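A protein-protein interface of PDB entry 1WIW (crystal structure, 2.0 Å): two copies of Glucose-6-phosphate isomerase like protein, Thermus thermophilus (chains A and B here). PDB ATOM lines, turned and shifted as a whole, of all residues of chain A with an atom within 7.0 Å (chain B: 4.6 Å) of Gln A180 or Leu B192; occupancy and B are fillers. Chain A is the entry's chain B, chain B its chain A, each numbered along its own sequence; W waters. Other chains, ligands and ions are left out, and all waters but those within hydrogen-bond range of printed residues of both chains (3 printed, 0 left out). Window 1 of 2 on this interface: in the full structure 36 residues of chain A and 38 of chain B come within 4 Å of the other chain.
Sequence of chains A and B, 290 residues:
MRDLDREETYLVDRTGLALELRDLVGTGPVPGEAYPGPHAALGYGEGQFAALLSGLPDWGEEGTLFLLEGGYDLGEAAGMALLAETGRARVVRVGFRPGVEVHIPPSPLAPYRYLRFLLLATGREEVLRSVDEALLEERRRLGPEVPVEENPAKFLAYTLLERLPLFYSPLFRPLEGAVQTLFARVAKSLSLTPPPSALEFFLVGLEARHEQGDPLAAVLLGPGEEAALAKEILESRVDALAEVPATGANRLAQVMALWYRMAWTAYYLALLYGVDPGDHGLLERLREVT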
ATOM      1  N   LEU A 164     -13.070 -11.822  20.017  1.00  0.00           N
ATOM      2  CA  LEU A 164     -13.740 -11.255  21.177  1.00  0.00           C
ATOM      3  C   LEU A 164     -12.630 -10.855  22.137  1.00  0.00           C
ATOM      4  O   LEU A 164     -12.050 -11.703  22.810  1.00  0.00           O
ATOM      5  CB  LEU A 164     -14.647 -12.300  21.837  1.00  0.00           C
ATOM      6  CG  LEU A 164     -15.357 -11.866  23.121  1.00  0.00           C
ATOM      7  CD1 LEU A 164     -16.211 -10.638  22.844  1.00  0.00           C
ATOM      8  CD2 LEU A 164     -16.220 -13.013  23.649  1.00  0.00           C
ATOM      9  N   PRO A 165     -12.295  -9.559  22.188  1.00  0.00           N
ATOM     10  CA  PRO A 165     -11.228  -9.130  23.093  1.00  0.00           C
ATOM     11  C   PRO A 165     -11.563  -9.202  24.576  1.00  0.00           C
ATOM     12  O   PRO A 165     -12.677  -8.896  25.006  1.00  0.00           O
ATOM     13  CB  PRO A 165     -10.915  -7.705  22.622  1.00  0.00           C
ATOM     14  CG  PRO A 165     -12.199  -7.241  22.040  1.00  0.00           C
ATOM     15  CD  PRO A 165     -12.739  -8.453  21.321  1.00  0.00           C
ATOM     16  N   PHE A 167     -10.078  -7.682  27.918  1.00  0.00           N
ATOM     17  CA  PHE A 167      -9.171  -6.683  28.474  1.00  0.00           C
ATOM     18  C   PHE A 167      -8.917  -6.873  29.964  1.00  0.00           C
ATOM     19  O   PHE A 167      -9.858  -7.001  30.750  1.00  0.00           O
ATOM     20  CB  PHE A 167      -9.723  -5.273  28.248  1.00  0.00           C
ATOM     21  CG  PHE A 167      -9.981  -4.940  26.807  1.00  0.00           C
ATOM     22  CD1 PHE A 167     -11.280  -4.814  26.330  1.00  0.00           C
ATOM     23  CD2 PHE A 167      -8.927  -4.735  25.929  1.00  0.00           C
ATOM     24  CE1 PHE A 167     -11.523  -4.485  24.995  1.00  0.00           C
ATOM     25  CE2 PHE A 167      -9.159  -4.406  24.594  1.00  0.00           C
ATOM     26  CZ  PHE A 167     -10.462  -4.280  24.128  1.00  0.00           C
ATOM     27  N   LEU A 175      -9.793   0.466  34.408  1.00  0.00           N
ATOM     28  CA  LEU A 175      -9.407   0.780  33.034  1.00  0.00           C
ATOM     29  C   LEU A 175     -10.090  -0.181  32.053  1.00  0.00           C
ATOM     30  O   LEU A 175     -10.510   0.229  30.969  1.00  0.00           O
ATOM     31  CB  LEU A 175      -7.884   0.698  32.857  1.00  0.00           C
ATOM     32  CG  LEU A 175      -7.367   0.825  31.410  1.00  0.00           C
ATOM     33  CD1 LEU A 175      -7.796   2.164  30.812  1.00  0.00           C
ATOM     34  CD2 LEU A 175      -5.844   0.693  31.388  1.00  0.00           C
ATOM     35  N   GLU A 176     -10.201  -1.450  32.441  1.00  0.00           N
ATOM     36  CA  GLU A 176     -10.830  -2.475  31.597  1.00  0.00           C
ATOM     37  C   GLU A 176     -12.221  -2.039  31.148  1.00  0.00           C
ATOM     38  O   GLU A 176     -12.566  -2.128  29.966  1.00  0.00           O
ATOM     39  CB  GLU A 176     -10.942  -3.793  32.370  1.00  0.00           C
ATOM     40  CG  GLU A 176      -9.603  -4.350  32.810  1.00  0.00           C
ATOM     41  CD  GLU A 176      -9.718  -5.324  33.966  1.00  0.00           C
ATOM     42  OE1 GLU A 176      -8.669  -5.811  34.421  1.00  0.00           O
ATOM     43  OE2 GLU A 176     -10.849  -5.596  34.421  1.00  0.00           O
ATOM     44  N   GLY A 177     -13.016  -1.577  32.108  1.00  0.00           N
ATOM     45  CA  GLY A 177     -14.361  -1.124  31.812  1.00  0.00           C
ATOM     46  C   GLY A 177     -14.361   0.060  30.865  1.00  0.00           C
ATOM     47  O   GLY A 177     -15.187   0.129  29.960  1.00  0.00           O
ATOM     48  N   ALA A 178     -13.434   0.991  31.065  1.00  0.00           N
ATOM     49  CA  ALA A 178     -13.358   2.166  30.204  1.00  0.00           C
ATOM     50  C   ALA A 178     -12.978   1.776  28.773  1.00  0.00           C
ATOM     51  O   ALA A 178     -13.474   2.368  27.810  1.00  0.00           O
ATOM     52  CB  ALA A 178     -12.341   3.165  30.765  1.00  0.00           C
ATOM     53  N   VAL A 179     -12.087   0.794  28.637  1.00  0.00           N
ATOM     54  CA  VAL A 179     -11.665   0.341  27.318  1.00  0.00           C
ATOM     55  C   VAL A 179     -12.779  -0.466  26.662  1.00  0.00           C
ATOM     56  O   VAL A 179     -12.987  -0.381  25.448  1.00  0.00           O
ATOM     57  CB  VAL A 179     -10.370  -0.504  27.385  1.00  0.00           C
ATOM     58  CG1 VAL A 179     -10.090  -1.139  26.023  1.00  0.00           C
ATOM     59  CG2 VAL A 179      -9.181   0.393  27.778  1.00  0.00           C
ATOM     60  N   GLN A 180     -13.495  -1.252  27.461  1.00  0.00           N
ATOM     61  CA  GLN A 180     -14.615  -2.038  26.938  1.00  0.00           C
ATOM     62  C   GLN A 180     -15.601  -1.047  26.321  1.00  0.00           C
ATOM     63  O   GLN A 180     -16.175  -1.296  25.257  1.00  0.00           O
ATOM     64  CB  GLN A 180     -15.304  -2.809  28.069  1.00  0.00           C
ATOM     65  CG  GLN A 180     -16.437  -3.731  27.616  1.00  0.00           C
ATOM     66  CD  GLN A 180     -17.076  -4.482  28.777  1.00  0.00           C
ATOM     67  OE1 GLN A 180     -17.744  -5.503  28.584  1.00  0.00           O
ATOM     68  NE2 GLN A 180     -16.884  -3.974  29.987  1.00  0.00           N
ATOM     69  N   THR A 181     -15.786   0.083  27.002  1.00  0.00           N
ATOM     70  CA  THR A 181     -16.688   1.131  26.535  1.00  0.00           C
ATOM     71  C   THR A 181     -16.193   1.777  25.243  1.00  0.00           C
ATOM     72  O   THR A 181     -16.992   2.096  24.353  1.00  0.00           O
ATOM     73  CB  THR A 181     -16.878   2.210  27.626  1.00  0.00           C
ATOM     74  OG1 THR A 181     -17.728   1.692  28.655  1.00  0.00           O
ATOM     75  CG2 THR A 181     -17.504   3.478  27.053  1.00  0.00           C
ATOM     76  N   LEU A 182     -14.880   1.975  25.135  1.00  0.00           N
ATOM     77  CA  LEU A 182     -14.312   2.569  23.925  1.00  0.00           C
ATOM     78  C   LEU A 182     -14.581   1.678  22.712  1.00  0.00           C
ATOM     79  O   LEU A 182     -14.920   2.166  21.638  1.00  0.00           O
ATOM     80  CB  LEU A 182     -12.797   2.772  24.076  1.00  0.00           C
ATOM     81  CG  LEU A 182     -12.348   4.012  24.855  1.00  0.00           C
ATOM     82  CD1 LEU A 182     -10.858   3.946  25.145  1.00  0.00           C
ATOM     83  CD2 LEU A 182     -12.685   5.265  24.047  1.00  0.00           C
ATOM     84  N   PHE A 183     -14.431   0.370  22.888  1.00  0.00           N
ATOM     85  CA  PHE A 183     -14.652  -0.565  21.789  1.00  0.00           C
ATOM     86  C   PHE A 183     -16.110  -0.699  21.373  1.00  0.00           C
ATOM     87  O   PHE A 183     -16.411  -1.030  20.223  1.00  0.00           O
ATOM     88  CB  PHE A 183     -14.050  -1.926  22.134  1.00  0.00           C
ATOM     89  CG  PHE A 183     -12.583  -2.015  21.816  1.00  0.00           C
ATOM     90  CD1 PHE A 183     -12.153  -2.540  20.602  1.00  0.00           C
ATOM     91  CD2 PHE A 183     -11.641  -1.470  22.680  1.00  0.00           C
ATOM     92  CE1 PHE A 183     -10.804  -2.516  20.246  1.00  0.00           C
ATOM     93  CE2 PHE A 183     -10.289  -1.439  22.339  1.00  0.00           C
ATOM     94  CZ  PHE A 183      -9.870  -1.963  21.117  1.00  0.00           C
ATOM     95  N   ALA A 184     -17.020  -0.436  22.298  1.00  0.00           N
ATOM     96  CA  ALA A 184     -18.433  -0.514  21.961  1.00  0.00           C
ATOM     97  C   ALA A 184     -18.847   0.788  21.276  1.00  0.00           C
ATOM     98  O   ALA A 184     -19.484   0.768  20.224  1.00  0.00           O
ATOM     99  CB  ALA A 184     -19.274  -0.739  23.214  1.00  0.00           C
ATOM    100  N   ARG A 185     -18.457   1.922  21.849  1.00  0.00           N
ATOM    101  CA  ARG A 185     -18.868   3.192  21.264  1.00  0.00           C
ATOM    102  C   ARG A 185     -18.172   3.589  19.971  1.00  0.00           C
ATOM    103  O   ARG A 185     -18.802   4.159  19.078  1.00  0.00           O
ATOM    104  CB  ARG A 185     -18.735   4.346  22.261  1.00  0.00           C
ATOM    105  CG  ARG A 185     -19.585   5.522  21.794  1.00  0.00           C
ATOM    106  CD  ARG A 185     -19.085   6.882  22.202  1.00  0.00           C
ATOM    107  NE  ARG A 185     -19.343   7.174  23.599  1.00  0.00           N
ATOM    108  CZ  ARG A 185     -19.698   8.372  24.048  1.00  0.00           C
ATOM    109  NH1 ARG A 185     -19.906   8.554  25.343  1.00  0.00           N
ATOM    110  NH2 ARG A 185     -19.864   9.379  23.200  1.00  0.00           N
ATOM    111  N   SER A 189     -18.141  -2.711  18.638  1.00  0.00           N
ATOM    112  CA  SER A 189     -17.870  -4.129  18.846  1.00  0.00           C
ATOM    113  C   SER A 189     -17.908  -4.573  20.300  1.00  0.00           C
ATOM    114  O   SER A 189     -17.666  -3.795  21.219  1.00  0.00           O
ATOM    115  CB  SER A 189     -16.502  -4.493  18.249  1.00  0.00           C
ATOM    116  OG  SER A 189     -16.457  -4.216  16.856  1.00  0.00           O
ATOM    117  N   LEU A 190     -18.200  -5.853  20.483  1.00  0.00           N
ATOM    118  CA  LEU A 190     -18.296  -6.471  21.792  1.00  0.00           C
ATOM    119  C   LEU A 190     -16.916  -6.865  22.319  1.00  0.00           C
ATOM    120  O   LEU A 190     -16.038  -7.241  21.550  1.00  0.00           O
ATOM    121  CB  LEU A 190     -19.176  -7.720  21.684  1.00  0.00           C
ATOM    122  CG  LEU A 190     -19.507  -8.516  22.943  1.00  0.00           C
ATOM    123  CD1 LEU A 190     -20.427  -7.692  23.825  1.00  0.00           C
ATOM    124  CD2 LEU A 190     -20.182  -9.836  22.560  1.00  0.00           C
ATOM    125  N   SER A 191     -16.740  -6.769  23.633  1.00  0.00           N
ATOM    126  CA  SER A 191     -15.503  -7.155  24.303  1.00  0.00           C
ATOM    127  C   SER A 191     -15.887  -7.451  25.743  1.00  0.00           C
ATOM    128  O   SER A 191     -17.007  -7.151  26.163  1.00  0.00           O
ATOM    129  CB  SER A 191     -14.460  -6.031  24.262  1.00  0.00           C
ATOM    130  OG  SER A 191     -14.888  -4.887  24.984  1.00  0.00           O
ATOM    131  N   LEU A 192     -14.986  -8.058  26.504  1.00  0.00           N
ATOM    132  CA  LEU A 192     -15.318  -8.327  27.894  1.00  0.00           C
ATOM    133  C   LEU A 192     -14.176  -8.070  28.845  1.00  0.00           C
ATOM    134  O   LEU A 192     -13.026  -7.892  28.443  1.00  0.00           O
ATOM    135  CB  LEU A 192     -15.806  -9.760  28.098  1.00  0.00           C
ATOM    136  CG  LEU A 192     -14.749 -10.854  28.151  1.00  0.00           C
ATOM    137  CD1 LEU A 192     -15.285 -12.049  28.940  1.00  0.00           C
ATOM    138  CD2 LEU A 192     -14.361 -11.240  26.741  1.00  0.00           C
ATOM    139  N   THR A 193     -14.531  -8.083  30.121  1.00  0.00           N
ATOM    140  CA  THR A 193     -13.613  -7.848  31.216  1.00  0.00           C
ATOM    141  C   THR A 193     -13.744  -8.993  32.209  1.00  0.00           C
ATOM    142  O   THR A 193     -14.805  -9.608  32.325  1.00  0.00           O
ATOM    143  CB  THR A 193     -13.982  -6.536  31.930  1.00  0.00           C
ATOM    144  OG1 THR A 193     -13.657  -5.432  31.076  1.00  0.00           O
ATOM    145  CG2 THR A 193     -13.247  -6.404  33.249  1.00  0.00           C
ATOM    146  N   PHE A 201     -10.471 -16.557  37.428  1.00  0.00           N
ATOM    147  CA  PHE A 201     -11.358 -16.588  36.275  1.00  0.00           C
ATOM    148  C   PHE A 201     -10.631 -17.159  35.051  1.00  0.00           C
ATOM    149  O   PHE A 201     -11.159 -18.027  34.343  1.00  0.00           O
ATOM    150  CB  PHE A 201     -11.842 -15.162  35.993  1.00  0.00           C
ATOM    151  CG  PHE A 201     -12.669 -15.023  34.748  1.00  0.00           C
ATOM    152  CD1 PHE A 201     -13.990 -15.456  34.717  1.00  0.00           C
ATOM    153  CD2 PHE A 201     -12.132 -14.431  33.610  1.00  0.00           C
ATOM    154  CE1 PHE A 201     -14.768 -15.299  33.571  1.00  0.00           C
ATOM    155  CE2 PHE A 201     -12.900 -14.270  32.456  1.00  0.00           C
ATOM    156  CZ  PHE A 201     -14.222 -14.706  32.440  1.00  0.00           C
ATOM    157  N   PRO B 165     -23.495 -16.106  28.079  1.00  0.00           N
ATOM    158  CA  PRO B 165     -24.272 -15.286  29.012  1.00  0.00           C
ATOM    159  C   PRO B 165     -23.752 -13.862  29.174  1.00  0.00           C
ATOM    160  O   PRO B 165     -22.544 -13.639  29.282  1.00  0.00           O
ATOM    161  CB  PRO B 165     -24.176 -16.056  30.333  1.00  0.00           C
ATOM    162  CG  PRO B 165     -23.809 -17.449  29.926  1.00  0.00           C
ATOM    163  CD  PRO B 165     -22.860 -17.235  28.781  1.00  0.00           C
ATOM    164  N   LEU B 166     -24.685 -12.915  29.192  1.00  0.00           N
ATOM    165  CA  LEU B 166     -24.391 -11.499  29.391  1.00  0.00           C
ATOM    166  C   LEU B 166     -25.255 -11.106  30.589  1.00  0.00           C
ATOM    167  O   LEU B 166     -26.479 -10.998  30.476  1.00  0.00           O
ATOM    168  CB  LEU B 166     -24.787 -10.679  28.159  1.00  0.00           C
ATOM    169  CG  LEU B 166     -24.648  -9.151  28.239  1.00  0.00           C
ATOM    170  CD1 LEU B 166     -23.300  -8.743  28.814  1.00  0.00           C
ATOM    171  CD2 LEU B 166     -24.819  -8.572  26.846  1.00  0.00           C
ATOM    172  N   PHE B 167     -24.614 -10.912  31.737  1.00  0.00           N
ATOM    173  CA  PHE B 167     -25.325 -10.571  32.960  1.00  0.00           C
ATOM    174  C   PHE B 167     -25.366  -9.064  33.227  1.00  0.00           C
ATOM    175  O   PHE B 167     -24.356  -8.375  33.102  1.00  0.00           O
ATOM    176  CB  PHE B 167     -24.669 -11.272  34.152  1.00  0.00           C
ATOM    177  CG  PHE B 167     -24.616 -12.769  34.031  1.00  0.00           C
ATOM    178  CD1 PHE B 167     -23.402 -13.421  33.852  1.00  0.00           C
ATOM    179  CD2 PHE B 167     -25.772 -13.532  34.143  1.00  0.00           C
ATOM    180  CE1 PHE B 167     -23.339 -14.817  33.793  1.00  0.00           C
ATOM    181  CE2 PHE B 167     -25.719 -14.928  34.086  1.00  0.00           C
ATOM    182  CZ  PHE B 167     -24.503 -15.568  33.912  1.00  0.00           C
ATOM    183  N   GLN B 180     -20.618 -13.642  37.319  1.00  0.00           N
ATOM    184  CA  GLN B 180     -19.630 -14.046  36.320  1.00  0.00           C
ATOM    185  C   GLN B 180     -18.632 -14.989  37.006  1.00  0.00           C
ATOM    186  O   GLN B 180     -18.171 -15.965  36.420  1.00  0.00           O
ATOM    187  CB  GLN B 180     -18.907 -12.811  35.768  1.00  0.00           C
ATOM    188  CG  GLN B 180     -17.797 -13.110  34.763  1.00  0.00           C
ATOM    189  CD  GLN B 180     -17.066 -11.852  34.325  1.00  0.00           C
ATOM    190  OE1 GLN B 180     -16.807 -10.959  35.134  1.00  0.00           O
ATOM    191  NE2 GLN B 180     -16.720 -11.780  33.041  1.00  0.00           N
ATOM    192  N   SER B 191     -18.551 -16.084  30.608  1.00  0.00           N
ATOM    193  CA  SER B 191     -19.716 -15.208  30.667  1.00  0.00           C
ATOM    194  C   SER B 191     -19.205 -13.769  30.682  1.00  0.00           C
ATOM    195  O   SER B 191     -18.052 -13.518  31.049  1.00  0.00           O
ATOM    196  CB  SER B 191     -20.572 -15.488  31.908  1.00  0.00           C
ATOM    197  OG  SER B 191     -19.938 -15.060  33.093  1.00  0.00           O
ATOM    198  N   LEU B 192     -20.067 -12.835  30.287  1.00  0.00           N
ATOM    199  CA  LEU B 192     -19.707 -11.422  30.194  1.00  0.00           C
ATOM    200  C   LEU B 192     -20.603 -10.479  30.996  1.00  0.00           C
ATOM    201  O   LEU B 192     -21.750 -10.809  31.314  1.00  0.00           O
ATOM    202  CB  LEU B 192     -19.724 -11.030  28.708  1.00  0.00           C
ATOM    203  CG  LEU B 192     -19.893  -9.590  28.216  1.00  0.00           C
ATOM    204  CD1 LEU B 192     -18.769  -8.714  28.722  1.00  0.00           C
ATOM    205  CD2 LEU B 192     -19.905  -9.591  26.696  1.00  0.00           C
ATOM    206  N   THR B 193     -20.056  -9.309  31.331  1.00  0.00           N
ATOM    207  CA  THR B 193     -20.777  -8.273  32.067  1.00  0.00           C
ATOM    208  C   THR B 193     -20.499  -6.959  31.340  1.00  0.00           C
ATOM    209  O   THR B 193     -19.409  -6.748  30.801  1.00  0.00           O
ATOM    210  CB  THR B 193     -20.292  -8.114  33.535  1.00  0.00           C
ATOM    211  OG1 THR B 193     -19.038  -7.415  33.556  1.00  0.00           O
ATOM    212  CG2 THR B 193     -20.115  -9.476  34.199  1.00  0.00           C
ATOM    213  N   PRO B 194     -21.482  -6.059  31.313  1.00  0.00           N
ATOM    214  CA  PRO B 194     -21.263  -4.784  30.627  1.00  0.00           C
ATOM    215  C   PRO B 194     -20.436  -3.810  31.463  1.00  0.00           C
ATOM    216  O   PRO B 194     -20.280  -3.993  32.671  1.00  0.00           O
ATOM    217  CB  PRO B 194     -22.681  -4.286  30.394  1.00  0.00           C
ATOM    218  CG  PRO B 194     -23.390  -4.755  31.635  1.00  0.00           C
ATOM    219  CD  PRO B 194     -22.866  -6.167  31.811  1.00  0.00           C
ATOM    220  N   PRO B 195     -19.887  -2.765  30.826  1.00  0.00           N
ATOM    221  CA  PRO B 195     -19.090  -1.780  31.560  1.00  0.00           C
ATOM    222  C   PRO B 195     -20.040  -0.861  32.332  1.00  0.00           C
ATOM    223  O   PRO B 195     -21.260  -1.011  32.240  1.00  0.00           O
ATOM    224  CB  PRO B 195     -18.354  -1.048  30.447  1.00  0.00           C
ATOM    225  CG  PRO B 195     -19.374  -1.042  29.346  1.00  0.00           C
ATOM    226  CD  PRO B 195     -19.892  -2.466  29.383  1.00  0.00           C
ATOM    227  N   PHE B 201     -23.385   0.558  26.012  1.00  0.00           N
ATOM    228  CA  PHE B 201     -22.700  -0.659  25.553  1.00  0.00           C
ATOM    229  C   PHE B 201     -23.648  -1.565  24.760  1.00  0.00           C
ATOM    230  O   PHE B 201     -23.285  -2.091  23.707  1.00  0.00           O
ATOM    231  CB  PHE B 201     -22.155  -1.397  26.792  1.00  0.00           C
ATOM    232  CG  PHE B 201     -21.513  -2.735  26.504  1.00  0.00           C
ATOM    233  CD1 PHE B 201     -20.223  -2.815  25.983  1.00  0.00           C
ATOM    234  CD2 PHE B 201     -22.185  -3.917  26.807  1.00  0.00           C
ATOM    235  CE1 PHE B 201     -19.611  -4.053  25.773  1.00  0.00           C
ATOM    236  CE2 PHE B 201     -21.584  -5.155  26.602  1.00  0.00           C
ATOM    237  CZ  PHE B 201     -20.295  -5.225  26.085  1.00  0.00           C
HETATM  238  O   HOH W   1     -17.289  -5.175  32.277  1.00  0.00           O
HETATM  239  O   HOH W   2     -16.816  -8.412  34.429  1.00  0.00           O
HETATM  240  O   HOH W   3     -17.119  -8.575  31.016  1.00  0.00           O
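The side-chain amide nitrogen of Gln A180 sits close to the backbone nitrogen of Pro B195 (3.3 Å). The backbone carbonyl oxygen of Thr A193 sits at hydrogen-bond distance from the side-chain amide nitrogen of Gln B180 (3.0 Å). The backbone carbonyl oxygen (O) of Thr B193 lies close to the side-chain amide oxygen (OE1) of Gln A180.
The backbone carbonyl oxygen (O) of Pro B165 is in hydrogen-bond range of the backbone NH (N) of Leu B192, 2.8 Å away. The side-chain amide oxygen (OE1) of Gln A180 sits close to the backbone carbonyl oxygen (O) of Ser A191. N of Leu A192 is in hydrogen-bond range of O of Pro A165, 2.9 Å away. The backbone NH (N) of Phe B167 lies within hydrogen-bond range of the backbone carbonyl oxygen (O) of Leu B192 (2.9 Å). O of Gly A177 lies within hydrogen-bond range of OG1 of Thr A181, at 3.3 Å. The side-chain amide nitrogen of Gln B180 sits at hydrogen-bond distance from the backbone carbonyl oxygen of Ser B191.
Pro B195 touches Gly A177. Leu B192 touches Gln A180. Pro B194 touches Gln A180 (C to NE2, 3.8 Å). Phe B201 touches Gln A180 (CZ to OE1, 3.6 Å). CG of Pro B195 touches OG1 of Thr A181, at 3.3 Å. Phe B201 touches Ala A184. Leu B192 touches Leu A190 (CD2 to CD1, 3.5 Å). Ser A191 touches Leu B192. Ser A191 touches Phe B201. Leu A192 touches Leu B192 (CB to CD1, 3.2 Å).
Leu A175 touches none of the printed residues of chain B. Of the printed residues of chain B, Gln A180 touches Leu B192, Thr B193, Pro B194, Pro B195 and Phe B201. Of the printed residues of chain B, Leu A190 touches Leu B192 and Phe B201. Printed residues of chain A within 4 Å of Gln B180: Thr A193 and Phe A201. Printed residues of chain A within 4 Å of Leu B192: Gln A180, Leu A190, Ser A191 and Leu A192. Printed residues of chain A within 4 Å of Thr B193: Gln A180. The nearest printed residue of chain B that does not touch Gln A180 is Leu B166 (6.4 Å). The nearest printed residue of chain B that does not touch Thr A193 is Leu B192 (4.5 Å).
Hydrophobic or aromatic side chains of chain A within 4 Å of the printed part of chain B: Ala A184, Leu A190, Leu A192 and Phe A201. Printed residues of chain B that touch a printed residue of chain A: Gln B180, Ser B191, Leu B192, Thr B193, Pro B194, Pro B195 and Phe B201. Hydrophobic or aromatic side chains of chain B that line the printed part of chain A: Leu B192, Pro B195 and Phe B201.
Gln A180 touches Leu B192, but with the chains exchanged Leu A192 does not touch Gln B180 (4.4 Å). Gln A180 touches Thr B193, and with the chains exchanged Thr A193 touches Gln B180. Gln A180 touches Phe B201, and with the chains exchanged Phe A201 touches Gln B180. Ser A191 touches Phe B201, but with the chains exchanged Phe A201 does not touch Ser B191 (4.2 Å). Positions printed for both chains: 165, 167, 180, 191, 192, 193 and 201. Of the 16 pairs that touch across the chains among the printed residues, 7 have their exchanged pair printed and touching as well.
Water W2 lies within hydrogen-bond range of OG1 of Thr B193 (2.6 Å), OE1 of Gln B180 (2.6 Å) and O of Thr A193 (3.1 Å). Water W1 lies within hydrogen-bond range of NE2 of Gln A180 (2.6 Å), O of Thr B193 (3.0 Å) and O of Pro B194 (3.2 Å). Water W3 lies within hydrogen-bond range of N of Thr A193 and O of Thr B193.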
